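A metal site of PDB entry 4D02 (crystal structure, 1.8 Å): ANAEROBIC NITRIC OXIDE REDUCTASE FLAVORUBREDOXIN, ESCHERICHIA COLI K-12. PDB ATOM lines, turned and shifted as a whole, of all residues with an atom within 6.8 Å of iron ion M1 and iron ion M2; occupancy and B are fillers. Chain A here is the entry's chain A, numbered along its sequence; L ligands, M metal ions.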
ATOM      1  N   PHE A  22       0.767  27.267   4.969  1.00  0.00           N
ATOM      2  CA  PHE A  22       2.047  27.651   4.406  1.00  0.00           C
ATOM      3  C   PHE A  22       1.791  28.557   3.218  1.00  0.00           C
ATOM      4  O   PHE A  22       0.778  28.385   2.529  1.00  0.00           O
ATOM      5  CB  PHE A  22       2.834  26.412   3.957  1.00  0.00           C
ATOM      6  CG  PHE A  22       4.023  26.100   4.813  1.00  0.00           C
ATOM      7  CD1 PHE A  22       3.855  25.501   6.050  1.00  0.00           C
ATOM      8  CD2 PHE A  22       5.302  26.387   4.363  1.00  0.00           C
ATOM      9  CE1 PHE A  22       4.959  25.199   6.844  1.00  0.00           C
ATOM     10  CE2 PHE A  22       6.403  26.094   5.155  1.00  0.00           C
ATOM     11  CZ  PHE A  22       6.231  25.496   6.401  1.00  0.00           C
ATOM     12  N   HIS A  23       2.697  29.493   2.965  1.00  0.00           N
ATOM     13  CA  HIS A  23       2.550  30.424   1.856  1.00  0.00           C
ATOM     14  C   HIS A  23       1.198  31.128   1.905  1.00  0.00           C
ATOM     15  O   HIS A  23       0.408  31.029   0.971  1.00  0.00           O
ATOM     16  CB  HIS A  23       2.710  29.695   0.516  1.00  0.00           C
ATOM     17  CG  HIS A  23       4.057  29.093   0.305  1.00  0.00           C
ATOM     18  ND1 HIS A  23       4.288  28.071  -0.592  1.00  0.00           N
ATOM     19  CD2 HIS A  23       5.254  29.373   0.871  1.00  0.00           C
ATOM     20  CE1 HIS A  23       5.567  27.747  -0.568  1.00  0.00           C
ATOM     21  NE2 HIS A  23       6.175  28.513   0.311  1.00  0.00           N
ATOM     22  N   TYR A  35      11.296  21.937  10.438  1.00  0.00           N
ATOM     23  CA  TYR A  35      12.356  22.727   9.823  1.00  0.00           C
ATOM     24  C   TYR A  35      13.681  22.138  10.263  1.00  0.00           C
ATOM     25  O   TYR A  35      14.085  22.269  11.418  1.00  0.00           O
ATOM     26  CB  TYR A  35      12.224  24.207  10.215  1.00  0.00           C
ATOM     27  CG  TYR A  35      10.781  24.628  10.214  1.00  0.00           C
ATOM     28  CD1 TYR A  35      10.090  24.845   9.031  1.00  0.00           C
ATOM     29  CD2 TYR A  35      10.092  24.780  11.409  1.00  0.00           C
ATOM     30  CE1 TYR A  35       8.748  25.189   9.031  1.00  0.00           C
ATOM     31  CE2 TYR A  35       8.752  25.138  11.419  1.00  0.00           C
ATOM     32  CZ  TYR A  35       8.079  25.339  10.236  1.00  0.00           C
ATOM     33  OH  TYR A  35       6.746  25.694  10.260  1.00  0.00           O
ATOM     34  N   HIS A  79      19.143  28.314   1.186  1.00  0.00           N
ATOM     35  CA  HIS A  79      17.867  28.836   0.689  1.00  0.00           C
ATOM     36  C   HIS A  79      17.349  29.794   1.745  1.00  0.00           C
ATOM     37  O   HIS A  79      17.333  29.463   2.918  1.00  0.00           O
ATOM     38  CB  HIS A  79      16.928  27.649   0.426  1.00  0.00           C
ATOM     39  CG  HIS A  79      15.523  28.015   0.052  1.00  0.00           C
ATOM     40  ND1 HIS A  79      15.225  28.969  -0.896  1.00  0.00           N
ATOM     41  CD2 HIS A  79      14.342  27.499   0.470  1.00  0.00           C
ATOM     42  CE1 HIS A  79      13.914  29.041  -1.038  1.00  0.00           C
ATOM     43  NE2 HIS A  79      13.355  28.163  -0.218  1.00  0.00           N
ATOM     44  N   GLU A  81      14.365  31.447   2.189  1.00  0.00           N
ATOM     45  CA  GLU A  81      12.958  31.587   2.558  1.00  0.00           C
ATOM     46  C   GLU A  81      12.815  31.562   4.090  1.00  0.00           C
ATOM     47  O   GLU A  81      13.603  30.926   4.786  1.00  0.00           O
ATOM     48  CB  GLU A  81      12.114  30.490   1.913  1.00  0.00           C
ATOM     49  CG  GLU A  81      10.623  30.768   1.957  1.00  0.00           C
ATOM     50  CD  GLU A  81       9.842  29.962   0.941  1.00  0.00           C
ATOM     51  OE1 GLU A  81      10.424  29.050   0.304  1.00  0.00           O
ATOM     52  OE2 GLU A  81       8.639  30.251   0.757  1.00  0.00           O
ATOM     53  N   ASP A  83      11.154  30.163   6.249  1.00  0.00           N
ATOM     54  CA  ASP A  83      11.011  28.943   7.021  1.00  0.00           C
ATOM     55  C   ASP A  83      12.362  28.252   7.234  1.00  0.00           C
ATOM     56  O   ASP A  83      12.443  27.259   7.948  1.00  0.00           O
ATOM     57  CB  ASP A  83      10.004  27.984   6.348  1.00  0.00           C
ATOM     58  CG  ASP A  83      10.379  27.620   4.914  1.00  0.00           C
ATOM     59  OD1 ASP A  83      10.958  28.468   4.196  1.00  0.00           O
ATOM     60  OD2 ASP A  83      10.083  26.481   4.509  1.00  0.00           O
ATOM     61  N   HIS A  84      13.417  28.794   6.634  1.00  0.00           N
ATOM     62  CA  HIS A  84      14.761  28.238   6.834  1.00  0.00           C
ATOM     63  C   HIS A  84      15.780  29.271   7.301  1.00  0.00           C
ATOM     64  O   HIS A  84      16.611  28.966   8.151  1.00  0.00           O
ATOM     65  CB  HIS A  84      15.241  27.562   5.562  1.00  0.00           C
ATOM     66  CG  HIS A  84      14.308  26.491   5.095  1.00  0.00           C
ATOM     67  ND1 HIS A  84      14.031  25.379   5.857  1.00  0.00           N
ATOM     68  CD2 HIS A  84      13.540  26.389   3.984  1.00  0.00           C
ATOM     69  CE1 HIS A  84      13.148  24.633   5.227  1.00  0.00           C
ATOM     70  NE2 HIS A  84      12.835  25.221   4.088  1.00  0.00           N
ATOM     71  N   HIS A 147      13.660  25.689  -5.309  1.00  0.00           N
ATOM     72  CA  HIS A 147      12.590  26.309  -6.094  1.00  0.00           C
ATOM     73  C   HIS A 147      12.702  27.840  -6.188  1.00  0.00           C
ATOM     74  O   HIS A 147      11.836  28.498  -6.766  1.00  0.00           O
ATOM     75  CB  HIS A 147      11.232  25.935  -5.489  1.00  0.00           C
ATOM     76  CG  HIS A 147      11.024  26.467  -4.106  1.00  0.00           C
ATOM     77  ND1 HIS A 147      10.104  27.462  -3.823  1.00  0.00           N
ATOM     78  CD2 HIS A 147      11.630  26.165  -2.937  1.00  0.00           C
ATOM     79  CE1 HIS A 147      10.152  27.742  -2.529  1.00  0.00           C
ATOM     80  NE2 HIS A 147      11.064  26.970  -1.978  1.00  0.00           N
ATOM     81  N   TRP A 148      13.760  28.407  -5.607  1.00  0.00           N
ATOM     82  CA  TRP A 148      14.003  29.846  -5.672  1.00  0.00           C
ATOM     83  C   TRP A 148      15.305  30.127  -6.420  1.00  0.00           C
ATOM     84  O   TRP A 148      16.137  29.227  -6.548  1.00  0.00           O
ATOM     85  CB  TRP A 148      14.086  30.463  -4.273  1.00  0.00           C
ATOM     86  CG  TRP A 148      12.779  30.930  -3.712  1.00  0.00           C
ATOM     87  CD1 TRP A 148      11.523  30.649  -4.183  1.00  0.00           C
ATOM     88  CD2 TRP A 148      12.609  31.757  -2.547  1.00  0.00           C
ATOM     89  NE1 TRP A 148      10.580  31.268  -3.385  1.00  0.00           N
ATOM     90  CE2 TRP A 148      11.212  31.948  -2.382  1.00  0.00           C
ATOM     91  CE3 TRP A 148      13.483  32.362  -1.646  1.00  0.00           C
ATOM     92  CZ2 TRP A 148      10.682  32.726  -1.336  1.00  0.00           C
ATOM     93  CZ3 TRP A 148      12.961  33.129  -0.606  1.00  0.00           C
ATOM     94  CH2 TRP A 148      11.570  33.303  -0.468  1.00  0.00           C
ATOM     95  N   SER A 151      18.426  29.026  -4.346  1.00  0.00           N
ATOM     96  CA  SER A 151      18.517  27.658  -3.845  1.00  0.00           C
ATOM     97  C   SER A 151      19.800  26.930  -4.231  1.00  0.00           C
ATOM     98  O   SER A 151      20.271  26.999  -5.371  1.00  0.00           O
ATOM     99  CB  SER A 151      17.321  26.838  -4.325  1.00  0.00           C
ATOM    100  OG  SER A 151      16.093  27.424  -3.925  1.00  0.00           O
ATOM    101  N   ASN A 165      18.025  20.768   1.254  1.00  0.00           N
ATOM    102  CA  ASN A 165      17.047  21.802   1.617  1.00  0.00           C
ATOM    103  C   ASN A 165      15.651  21.342   1.201  1.00  0.00           C
ATOM    104  O   ASN A 165      15.279  20.215   1.502  1.00  0.00           O
ATOM    105  CB  ASN A 165      17.420  23.151   1.005  1.00  0.00           C
ATOM    106  CG  ASN A 165      16.655  24.318   1.629  1.00  0.00           C
ATOM    107  OD1 ASN A 165      15.661  24.792   1.079  1.00  0.00           O
ATOM    108  ND2 ASN A 165      17.103  24.779   2.785  1.00  0.00           N
ATOM    109  N   ASP A 166      14.879  22.195   0.523  1.00  0.00           N
ATOM    110  CA  ASP A 166      13.488  21.869   0.187  1.00  0.00           C
ATOM    111  C   ASP A 166      13.336  20.600  -0.664  1.00  0.00           C
ATOM    112  O   ASP A 166      12.372  19.842  -0.519  1.00  0.00           O
ATOM    113  CB  ASP A 166      12.813  23.039  -0.554  1.00  0.00           C
ATOM    114  CG  ASP A 166      12.353  24.171   0.367  1.00  0.00           C
ATOM    115  OD1 ASP A 166      12.019  23.929   1.551  1.00  0.00           O
ATOM    116  OD2 ASP A 166      12.318  25.319  -0.129  1.00  0.00           O
ATOM    117  N   HIS A 171       6.165  18.124   4.012  1.00  0.00           N
ATOM    118  CA  HIS A 171       5.607  18.649   5.262  1.00  0.00           C
ATOM    119  C   HIS A 171       4.894  17.534   5.995  1.00  0.00           C
ATOM    120  O   HIS A 171       3.773  17.163   5.665  1.00  0.00           O
ATOM    121  CB  HIS A 171       4.667  19.818   4.979  1.00  0.00           C
ATOM    122  CG  HIS A 171       5.344  20.970   4.301  1.00  0.00           C
ATOM    123  ND1 HIS A 171       6.411  21.635   4.870  1.00  0.00           N
ATOM    124  CD2 HIS A 171       5.131  21.561   3.106  1.00  0.00           C
ATOM    125  CE1 HIS A 171       6.819  22.588   4.060  1.00  0.00           C
ATOM    126  NE2 HIS A 171       6.050  22.572   2.979  1.00  0.00           N
ATOM    127  N   TYR A 194       3.405  17.714  -1.765  1.00  0.00           N
ATOM    128  CA  TYR A 194       4.475  18.685  -1.818  1.00  0.00           C
ATOM    129  C   TYR A 194       4.963  18.922  -3.253  1.00  0.00           C
ATOM    130  O   TYR A 194       5.002  20.067  -3.727  1.00  0.00           O
ATOM    131  CB  TYR A 194       5.591  18.171  -0.941  1.00  0.00           C
ATOM    132  CG  TYR A 194       6.756  19.079  -0.721  1.00  0.00           C
ATOM    133  CD1 TYR A 194       7.866  19.024  -1.556  1.00  0.00           C
ATOM    134  CD2 TYR A 194       6.785  19.935   0.373  1.00  0.00           C
ATOM    135  CE1 TYR A 194       8.957  19.833  -1.331  1.00  0.00           C
ATOM    136  CE2 TYR A 194       7.871  20.746   0.607  1.00  0.00           C
ATOM    137  CZ  TYR A 194       8.952  20.689  -0.241  1.00  0.00           C
ATOM    138  OH  TYR A 194      10.038  21.499  -0.008  1.00  0.00           O
ATOM    139  N   ILE A 198       4.040  22.509  -5.196  1.00  0.00           N
ATOM    140  CA  ILE A 198       5.124  23.476  -5.132  1.00  0.00           C
ATOM    141  C   ILE A 198       6.102  23.332  -6.310  1.00  0.00           C
ATOM    142  O   ILE A 198       6.552  24.334  -6.889  1.00  0.00           O
ATOM    143  CB  ILE A 198       5.926  23.358  -3.805  1.00  0.00           C
ATOM    144  CG1 ILE A 198       4.986  23.390  -2.603  1.00  0.00           C
ATOM    145  CG2 ILE A 198       6.964  24.475  -3.697  1.00  0.00           C
ATOM    146  CD1 ILE A 198       4.311  24.705  -2.415  1.00  0.00           C
ATOM    147  N   SER A 226      15.362  19.807   4.325  1.00  0.00           N
ATOM    148  CA  SER A 226      15.031  20.856   5.271  1.00  0.00           C
ATOM    149  C   SER A 226      13.620  20.709   5.850  1.00  0.00           C
ATOM    150  O   SER A 226      13.206  21.497   6.702  1.00  0.00           O
ATOM    151  CB  SER A 226      15.199  22.215   4.611  1.00  0.00           C
ATOM    152  OG  SER A 226      14.294  22.353   3.534  1.00  0.00           O
ATOM    153  N   HIS A 227      12.886  19.703   5.362  1.00  0.00           N
ATOM    154  CA  HIS A 227      11.530  19.435   5.840  1.00  0.00           C
ATOM    155  C   HIS A 227      11.301  17.947   5.985  1.00  0.00           C
ATOM    156  O   HIS A 227      11.467  17.199   5.016  1.00  0.00           O
ATOM    157  CB  HIS A 227      10.465  19.983   4.881  1.00  0.00           C
ATOM    158  CG  HIS A 227      10.407  21.480   4.816  1.00  0.00           C
ATOM    159  ND1 HIS A 227       9.960  22.260   5.854  1.00  0.00           N
ATOM    160  CD2 HIS A 227      10.709  22.328   3.799  1.00  0.00           C
ATOM    161  CE1 HIS A 227      10.006  23.529   5.497  1.00  0.00           C
ATOM    162  NE2 HIS A 227      10.454  23.604   4.257  1.00  0.00           N
HETATM  163  O1  LIG L   1      11.483  27.017   2.061  1.00  0.00           O
HETATM  164  P1  LG2 L   2       8.527  25.692   1.176  1.00  0.00           P
HETATM  165  O1  LG2 L   2       8.004  26.758   2.123  1.00  0.00           O
HETATM  166  O2  LG2 L   2       9.251  26.361   0.032  1.00  0.00           O
HETATM  167  O3  LG2 L   2       9.484  24.776   1.891  1.00  0.00           O
HETATM  168  O4  LG2 L   2       7.381  24.874   0.651  1.00  0.00           O
HETATM  169  N1  LG3 L   3       8.901  36.082  -7.076  1.00  0.00           N
HETATM  170  C1  LG3 L   3       8.983  36.467  -8.394  1.00  0.00           C
HETATM  171  O1  LG3 L   3       9.559  37.516  -8.691  1.00  0.00           O
HETATM  172  N2  LG3 L   3       8.431  35.673  -9.388  1.00  0.00           N
HETATM  173  C2  LG3 L   3       7.788  34.498  -9.079  1.00  0.00           C
HETATM  174  O2  LG3 L   3       7.307  33.815  -9.992  1.00  0.00           O
HETATM  175  C3  LG3 L   3       7.683  34.099  -7.746  1.00  0.00           C
HETATM  176  N3  LG3 L   3       7.051  32.918  -7.397  1.00  0.00           N
HETATM  177  C4  LG3 L   3       6.958  32.545  -6.064  1.00  0.00           C
HETATM  178  C5  LG3 L   3       6.307  31.371  -5.703  1.00  0.00           C
HETATM  179  C6  LG3 L   3       6.213  30.998  -4.369  1.00  0.00           C
HETATM  180  C7  LG3 L   3       5.526  29.715  -3.974  1.00  0.00           C
HETATM  181  C8  LG3 L   3       6.791  31.797  -3.387  1.00  0.00           C
HETATM  182  C9  LG3 L   3       6.703  31.385  -1.933  1.00  0.00           C
HETATM  183  C10 LG3 L   3       7.438  32.972  -3.738  1.00  0.00           C
HETATM  184  C11 LG3 L   3       7.529  33.354  -5.075  1.00  0.00           C
HETATM  185  N4  LG3 L   3       8.167  34.525  -5.430  1.00  0.00           N
HETATM  186  C12 LG3 L   3       8.245  34.905  -6.760  1.00  0.00           C
HETATM  187  C13 LG3 L   3       8.790  35.418  -4.398  1.00  0.00           C
HETATM  188  C14 LG3 L   3       7.730  36.289  -3.725  1.00  0.00           C
HETATM  189  O3  LG3 L   3       7.048  37.090  -4.676  1.00  0.00           O
HETATM  190  C15 LG3 L   3       8.446  37.139  -2.678  1.00  0.00           C
HETATM  191  O4  LG3 L   3       8.784  36.279  -1.606  1.00  0.00           O
HETATM  192  C16 LG3 L   3       7.582  38.295  -2.207  1.00  0.00           C
HETATM  193  O5  LG3 L   3       8.361  39.192  -1.471  1.00  0.00           O
HETATM  194  C17 LG3 L   3       6.486  37.751  -1.314  1.00  0.00           C
HETATM  195  O6  LG3 L   3       5.579  38.785  -0.987  1.00  0.00           O
HETATM  196  P1  LG3 L   3       4.410  38.416   0.056  1.00  0.00           P
HETATM  197  O7  LG3 L   3       3.447  39.577   0.173  1.00  0.00           O
HETATM  198  O8  LG3 L   3       3.701  37.172  -0.417  1.00  0.00           O
HETATM  199  O9  LG3 L   3       5.063  38.147   1.396  1.00  0.00           O
HETATM  200 FE    FE M   1      11.052  25.187   2.912  1.00  0.00          FE
HETATM  201 FE    FE M   2      11.381  27.165   0.067  1.00  0.00          FE
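The backbone NH (N) of His 147 lies within hydrogen-bond range of the side-chain hydroxyl (OG) of Ser 151 (3.3 Å).
O of Asp 166 is in hydrogen-bond range of OH of Tyr 194, 2.9 Å away.
A ring nitrogen (NE2) of His 23 is in hydrogen-bond range of the side-chain carboxylate (OE2) of Glu 81, 3.0 Å away.
A ring nitrogen (NE2) of His 84 lies close to the side-chain hydroxyl (OG) of Ser 226 (3.3 Å).
The backbone NH of Asp 166 sits at hydrogen-bond distance from the side-chain hydroxyl of Ser 226, 3.1 Å away.
Within 4 Å of iron ion M1: Asp 83, His 84, Asp 166 and His 227.
Along chain A the residues within 4 Å of iron ion M1 span positions 83 to 227.
The nearest printed residue that does not touch iron ion M1 is Ser 226 (4.4 Å).
Of the 17 residues printed, 4 come within 4 Å of iron ion M2.
The nearest printed residue that does not touch iron ion M2 is Asp 83 (4.4 Å).
Iron ion M1 is bound by O3 of LG2 L2.
O1 of LIG L1 binds iron ion M1, 2.1 Å away.
Iron ion M1 is bound by the side-chain carboxylate (OD1) of Asp 166 (2.1 Å).
Iron ion M1 is bound by a ring nitrogen (NE2) of His 84 (2.1 Å).
Iron ion M1 is bound by NE2 of His 227 (2.2 Å).
OD2 of Asp 83 is bound to iron ion M1, at 2.3 Å.
Iron ion M2 is bound by an oxygen (O1) of LIG L1 (2.0 Å), a ring nitrogen (NE2) of His 147 (2.1 Å), the side-chain carboxylate (OD2) of Asp 166 (2.1 Å), the side-chain carboxylate (OE1) of Glu 81 (2.1 Å), a ring nitrogen (NE2) of His 79 (2.2 Å) and an oxygen (O2) of LG2 L2 (2.3 Å).
Iron ion M2 has six donor atoms within binding distance.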
